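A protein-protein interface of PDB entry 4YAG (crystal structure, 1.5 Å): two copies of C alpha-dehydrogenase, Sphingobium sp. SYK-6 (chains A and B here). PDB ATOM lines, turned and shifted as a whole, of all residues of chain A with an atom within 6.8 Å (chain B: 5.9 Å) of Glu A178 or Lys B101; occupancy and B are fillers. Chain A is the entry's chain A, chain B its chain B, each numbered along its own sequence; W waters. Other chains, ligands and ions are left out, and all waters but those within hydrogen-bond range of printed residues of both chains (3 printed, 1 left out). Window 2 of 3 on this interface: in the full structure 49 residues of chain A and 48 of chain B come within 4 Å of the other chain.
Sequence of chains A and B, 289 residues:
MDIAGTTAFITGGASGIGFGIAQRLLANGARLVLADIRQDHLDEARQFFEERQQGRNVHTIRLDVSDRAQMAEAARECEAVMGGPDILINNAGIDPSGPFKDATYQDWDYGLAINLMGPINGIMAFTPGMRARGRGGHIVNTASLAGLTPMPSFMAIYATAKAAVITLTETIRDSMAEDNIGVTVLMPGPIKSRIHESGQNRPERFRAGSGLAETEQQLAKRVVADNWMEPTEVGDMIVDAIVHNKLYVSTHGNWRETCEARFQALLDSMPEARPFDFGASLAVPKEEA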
ATOM      1  N   MET A 124      -6.984   3.816  24.176  1.00  0.00           N
ATOM      2  CA  MET A 124      -6.722   4.258  25.534  1.00  0.00           C
ATOM      3  C   MET A 124      -7.998   4.338  26.366  1.00  0.00           C
ATOM      4  O   MET A 124      -8.002   4.002  27.556  1.00  0.00           O
ATOM      5  CB  MET A 124      -6.016   5.616  25.509  1.00  0.00           C
ATOM      6  CG  MET A 124      -4.618   5.575  24.870  1.00  0.00           C
ATOM      7  SD  MET A 124      -3.423   4.506  25.717  1.00  0.00           S
ATOM      8  CE  MET A 124      -3.275   5.457  27.192  1.00  0.00           C
ATOM      9  N   ARG A 131     -10.168  -5.265  28.982  1.00  0.00           N
ATOM     10  CA  ARG A 131      -9.335  -6.164  29.765  1.00  0.00           C
ATOM     11  C   ARG A 131     -10.015  -6.525  31.084  1.00  0.00           C
ATOM     12  O   ARG A 131     -10.058  -7.692  31.476  1.00  0.00           O
ATOM     13  CB  ARG A 131      -7.990  -5.538  30.060  1.00  0.00           C
ATOM     14  CG  ARG A 131      -7.165  -5.139  28.855  1.00  0.00           C
ATOM     15  CD  ARG A 131      -5.852  -4.584  29.364  1.00  0.00           C
ATOM     16  NE  ARG A 131      -5.023  -3.907  28.372  1.00  0.00           N
ATOM     17  CZ  ARG A 131      -4.097  -4.503  27.616  1.00  0.00           C
ATOM     18  NH1 ARG A 131      -3.880  -5.811  27.726  1.00  0.00           N
ATOM     19  NH2 ARG A 131      -3.376  -3.781  26.774  1.00  0.00           N
ATOM     20  N   ARG A 173      -0.565  -5.982  19.308  1.00  0.00           N
ATOM     21  CA  ARG A 173      -1.141  -7.318  19.271  1.00  0.00           C
ATOM     22  C   ARG A 173      -0.782  -8.140  20.511  1.00  0.00           C
ATOM     23  O   ARG A 173      -1.636  -8.768  21.143  1.00  0.00           O
ATOM     24  CB  ARG A 173      -0.732  -8.066  17.993  1.00  0.00           C
ATOM     25  CG  ARG A 173      -1.461  -9.378  17.776  1.00  0.00           C
ATOM     26  CD  ARG A 173      -1.017 -10.046  16.487  1.00  0.00           C
ATOM     27  NE  ARG A 173      -2.084 -10.877  15.965  1.00  0.00           N
ATOM     28  CZ  ARG A 173      -1.956 -11.816  15.037  1.00  0.00           C
ATOM     29  NH1 ARG A 173      -0.761 -12.107  14.515  1.00  0.00           N
ATOM     30  NH2 ARG A 173      -3.039 -12.479  14.659  1.00  0.00           N
ATOM     31  N   ASP A 174       0.497  -8.180  20.863  1.00  0.00           N
ATOM     32  CA  ASP A 174       0.883  -9.063  21.952  1.00  0.00           C
ATOM     33  C   ASP A 174       0.322  -8.589  23.295  1.00  0.00           C
ATOM     34  O   ASP A 174      -0.046  -9.402  24.140  1.00  0.00           O
ATOM     35  CB  ASP A 174       2.404  -9.264  22.030  1.00  0.00           C
ATOM     36  CG  ASP A 174       3.145  -8.011  22.443  1.00  0.00           C
ATOM     37  OD1 ASP A 174       3.524  -7.241  21.551  1.00  0.00           O
ATOM     38  OD2 ASP A 174       3.376  -7.804  23.659  1.00  0.00           O
ATOM     39  N   SER A 175       0.251  -7.275  23.489  1.00  0.00           N
ATOM     40  CA  SER A 175      -0.327  -6.759  24.736  1.00  0.00           C
ATOM     41  C   SER A 175      -1.803  -7.114  24.829  1.00  0.00           C
ATOM     42  O   SER A 175      -2.291  -7.562  25.882  1.00  0.00           O
ATOM     43  CB  SER A 175      -0.170  -5.244  24.846  1.00  0.00           C
ATOM     44  OG  SER A 175      -0.744  -4.785  26.065  1.00  0.00           O
ATOM     45  N   MET A 176      -2.537  -6.900  23.741  1.00  0.00           N
ATOM     46  CA  MET A 176      -3.974  -7.172  23.769  1.00  0.00           C
ATOM     47  C   MET A 176      -4.241  -8.657  23.957  1.00  0.00           C
ATOM     48  O   MET A 176      -5.191  -9.056  24.638  1.00  0.00           O
ATOM     49  CB  MET A 176      -4.630  -6.661  22.490  1.00  0.00           C
ATOM     50  CG  MET A 176      -4.536  -5.147  22.337  1.00  0.00           C
ATOM     51  SD  MET A 176      -5.351  -4.274  23.716  1.00  0.00           S
ATOM     52  CE  MET A 176      -4.611  -2.654  23.565  1.00  0.00           C
ATOM     53  N   ALA A 177      -3.398  -9.479  23.356  1.00  0.00           N
ATOM     54  CA  ALA A 177      -3.555 -10.931  23.460  1.00  0.00           C
ATOM     55  C   ALA A 177      -3.443 -11.415  24.911  1.00  0.00           C
ATOM     56  O   ALA A 177      -3.998 -12.463  25.252  1.00  0.00           O
ATOM     57  CB  ALA A 177      -2.516 -11.638  22.614  1.00  0.00           C
ATOM     58  N   GLU A 178      -2.723 -10.687  25.762  1.00  0.00           N
ATOM     59  CA  GLU A 178      -2.642 -11.059  27.189  1.00  0.00           C
ATOM     60  C   GLU A 178      -4.033 -11.222  27.798  1.00  0.00           C
ATOM     61  O   GLU A 178      -4.230 -11.973  28.749  1.00  0.00           O
ATOM     62  CB  GLU A 178      -1.895  -9.984  27.989  1.00  0.00           C
ATOM     63  CG  GLU A 178      -0.464  -9.805  27.591  1.00  0.00           C
ATOM     64  CD  GLU A 178       0.175  -8.597  28.259  1.00  0.00           C
ATOM     65  OE1 GLU A 178      -0.417  -8.056  29.218  1.00  0.00           O
ATOM     66  OE2 GLU A 178       1.269  -8.198  27.824  1.00  0.00           O
ATOM     67  N   ASP A 179      -4.990 -10.475  27.268  1.00  0.00           N
ATOM     68  CA  ASP A 179      -6.351 -10.482  27.788  1.00  0.00           C
ATOM     69  C   ASP A 179      -7.346 -10.982  26.742  1.00  0.00           C
ATOM     70  O   ASP A 179      -8.533 -10.651  26.789  1.00  0.00           O
ATOM     71  CB  ASP A 179      -6.719  -9.076  28.272  1.00  0.00           C
ATOM     72  CG  ASP A 179      -5.923  -8.665  29.494  1.00  0.00           C
ATOM     73  OD1 ASP A 179      -6.228  -9.205  30.588  1.00  0.00           O
ATOM     74  OD2 ASP A 179      -4.993  -7.829  29.358  1.00  0.00           O
ATOM     75  N   ASN A 180      -6.851 -11.816  25.824  1.00  0.00           N
ATOM     76  CA  ASN A 180      -7.663 -12.461  24.803  1.00  0.00           C
ATOM     77  C   ASN A 180      -8.435 -11.442  23.970  1.00  0.00           C
ATOM     78  O   ASN A 180      -9.582 -11.666  23.576  1.00  0.00           O
ATOM     79  CB  ASN A 180      -8.608 -13.470  25.452  1.00  0.00           C
ATOM     80  CG  ASN A 180      -9.248 -14.402  24.444  1.00  0.00           C
ATOM     81  OD1 ASN A 180      -8.702 -14.647  23.360  1.00  0.00           O
ATOM     82  ND2 ASN A 180     -10.415 -14.936  24.796  1.00  0.00           N
ATOM     83  N   ILE A 181      -7.776 -10.323  23.694  1.00  0.00           N
ATOM     84  CA  ILE A 181      -8.287  -9.332  22.766  1.00  0.00           C
ATOM     85  C   ILE A 181      -7.465  -9.433  21.491  1.00  0.00           C
ATOM     86  O   ILE A 181      -6.247  -9.191  21.488  1.00  0.00           O
ATOM     87  CB  ILE A 181      -8.185  -7.920  23.354  1.00  0.00           C
ATOM     88  CG1 ILE A 181      -9.035  -7.797  24.629  1.00  0.00           C
ATOM     89  CG2 ILE A 181      -8.613  -6.865  22.317  1.00  0.00           C
ATOM     90  CD1 ILE A 181      -8.717  -6.555  25.447  1.00  0.00           C
ATOM     91  N   GLY B  98       8.255   1.166  26.983  1.00  0.00           N
ATOM     92  CA  GLY B  98       7.927   0.688  28.307  1.00  0.00           C
ATOM     93  C   GLY B  98       6.685  -0.178  28.224  1.00  0.00           C
ATOM     94  O   GLY B  98       6.035  -0.258  27.180  1.00  0.00           O
ATOM     95  N   PRO B  99       6.325  -0.824  29.332  1.00  0.00           N
ATOM     96  CA  PRO B  99       5.153  -1.702  29.349  1.00  0.00           C
ATOM     97  C   PRO B  99       3.913  -0.990  28.821  1.00  0.00           C
ATOM     98  O   PRO B  99       3.569   0.108  29.271  1.00  0.00           O
ATOM     99  CB  PRO B  99       5.005  -2.037  30.825  1.00  0.00           C
ATOM    100  CG  PRO B  99       6.354  -1.870  31.384  1.00  0.00           C
ATOM    101  CD  PRO B  99       6.921  -0.689  30.664  1.00  0.00           C
ATOM    102  N   PHE B 100       3.260  -1.595  27.829  1.00  0.00           N
ATOM    103  CA  PHE B 100       2.210  -0.912  27.101  1.00  0.00           C
ATOM    104  C   PHE B 100       1.065  -0.459  28.004  1.00  0.00           C
ATOM    105  O   PHE B 100       0.533   0.639  27.821  1.00  0.00           O
ATOM    106  CB  PHE B 100       1.672  -1.794  25.979  1.00  0.00           C
ATOM    107  CG  PHE B 100       0.662  -1.102  25.122  1.00  0.00           C
ATOM    108  CD1 PHE B 100       1.061  -0.270  24.106  1.00  0.00           C
ATOM    109  CD2 PHE B 100      -0.682  -1.228  25.379  1.00  0.00           C
ATOM    110  CE1 PHE B 100       0.128   0.389  23.325  1.00  0.00           C
ATOM    111  CE2 PHE B 100      -1.612  -0.565  24.617  1.00  0.00           C
ATOM    112  CZ  PHE B 100      -1.212   0.240  23.602  1.00  0.00           C
ATOM    113  N   LYS B 101       0.697  -1.287  28.982  1.00  0.00           N
ATOM    114  CA  LYS B 101      -0.414  -0.933  29.863  1.00  0.00           C
ATOM    115  C   LYS B 101      -0.071   0.237  30.784  1.00  0.00           C
ATOM    116  O   LYS B 101      -0.963   0.909  31.303  1.00  0.00           O
ATOM    117  CB  LYS B 101      -0.874  -2.147  30.669  1.00  0.00           C
ATOM    118  CG  LYS B 101      -1.382  -3.280  29.789  1.00  0.00           C
ATOM    119  CD  LYS B 101      -2.016  -4.409  30.601  1.00  0.00           C
ATOM    120  CE  LYS B 101      -1.031  -5.035  31.574  1.00  0.00           C
ATOM    121  NZ  LYS B 101       0.092  -5.744  30.891  1.00  0.00           N
ATOM    122  N   ASP B 102       1.213   0.502  30.973  1.00  0.00           N
ATOM    123  CA  ASP B 102       1.633   1.592  31.841  1.00  0.00           C
ATOM    124  C   ASP B 102       1.616   2.955  31.121  1.00  0.00           C
ATOM    125  O   ASP B 102       1.574   4.001  31.770  1.00  0.00           O
ATOM    126  CB  ASP B 102       3.025   1.319  32.396  1.00  0.00           C
ATOM    127  CG  ASP B 102       3.052   0.153  33.398  1.00  0.00           C
ATOM    128  OD1 ASP B 102       1.980  -0.383  33.752  1.00  0.00           O
ATOM    129  OD2 ASP B 102       4.160  -0.208  33.808  1.00  0.00           O
ATOM    130  N   ALA B 103       1.688   2.946  29.795  1.00  0.00           N
ATOM    131  CA  ALA B 103       1.819   4.178  29.035  1.00  0.00           C
ATOM    132  C   ALA B 103       0.554   5.012  29.191  1.00  0.00           C
ATOM    133  O   ALA B 103      -0.574   4.481  29.174  1.00  0.00           O
ATOM    134  CB  ALA B 103       2.071   3.876  27.562  1.00  0.00           C
ATOM    135  N   SER B 153       4.808  -4.787  21.820  1.00  0.00           N
ATOM    136  CA  SER B 153       4.033  -3.689  22.351  1.00  0.00           C
ATOM    137  C   SER B 153       4.814  -2.745  23.257  1.00  0.00           C
ATOM    138  O   SER B 153       4.449  -1.585  23.369  1.00  0.00           O
ATOM    139  CB  SER B 153       2.813  -4.245  23.104  1.00  0.00           C
ATOM    140  OG  SER B 153       3.273  -5.015  24.180  1.00  0.00           O
HETATM  141  O   HOH W   1       6.072  -6.293  24.553  1.00  0.00           O
HETATM  142  O   HOH W   2      -0.759   2.667  25.500  1.00  0.00           O
HETATM  143  O   HOH W   3       1.170  -5.404  27.796  1.00  0.00           O
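Of the printed residues of chain B, Met A124 touches Ala B103.
Printed residues of chain B within 4 Å of Met A176: Phe B100 (3.8 Å).
Glu A178 touches just one residue of chain B: Lys B101 (2.9 Å).
Gly B98 touches none of the printed residues of chain A.
Pro B99 touches none of the printed residues of chain A.
Printed residues of chain A within 4 Å of Phe B100: Arg A131, Ser A175 and Met A176.
Lys B101 touches just these residues of chain A: Arg A131 and Glu A178.
Of the printed residues of chain A, Ser B153 touches Asp A174 and Ser A175.
The nearest residue of chain B that does not touch Glu A178 is Ser B153 (5.2 Å).
The nearest residue of chain A that does not touch Lys B101 is Ser A175 (4.1 Å).
The nearest printed residue of chain B that does not touch Met A124 is Phe B100 (5.2 Å).
Met A124 touches Ala B103 (CE to O, 3.5 Å).
Phe B100 touches Arg A131 (CD2 to NH2, 3.97 Å).
CZ of Arg A131 touches CD of Lys B101, 3.6 Å away.
Ser A175 touches Phe B100.
CB of Ser A175 touches OG of Ser B153, 3.5 Å away.
Phe B100 touches Met A176 (CE2 to CE, 3.8 Å).
The guanidinium group of Arg A131 sits at hydrogen-bond distance from the side-chain hydroxyl of Ser A175 (2.9 Å).
The guanidinium group (NH2) of Arg A131 sits close to the side-chain sulfur (SD) of Met A176.
OD2 of Asp A179 is in salt-bridge range of NH1 of Arg A131, 2.8 Å away.
The backbone carbonyl oxygen (O) of Met A176 lies within hydrogen-bond range of the backbone NH (N) of Ile A181 (3.0 Å).
No position is printed for both chains.
N of Ser B153 lies within hydrogen-bond range of OD1 of Asp A174.
The side-chain carboxylate (OE1) of Glu A178 is in salt-bridge range of the side-chain amino group (NZ) of Lys B101, 2.9 Å away.
Water W3 lies within hydrogen-bond range of the side-chain hydroxyl of Ser A175 (2.7 Å), the side-chain carboxylate of Glu A178 (2.8 Å) and the side-chain amino group of Lys B101 (3.3 Å).
Water W1 bridges the side-chain hydroxyl of Ser B153 (3.1 Å) and the side-chain carboxylate of Asp A174 (3.2 Å).
Water W2 bridges SD of Met A124 (3.2 Å) and O of Phe B100 (3.3 Å).
Of the 11 printed residues of chain A, 6 touch a printed residue of chain B.
Of the 7 printed residues of chain B, 4 touch a printed residue of chain A.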
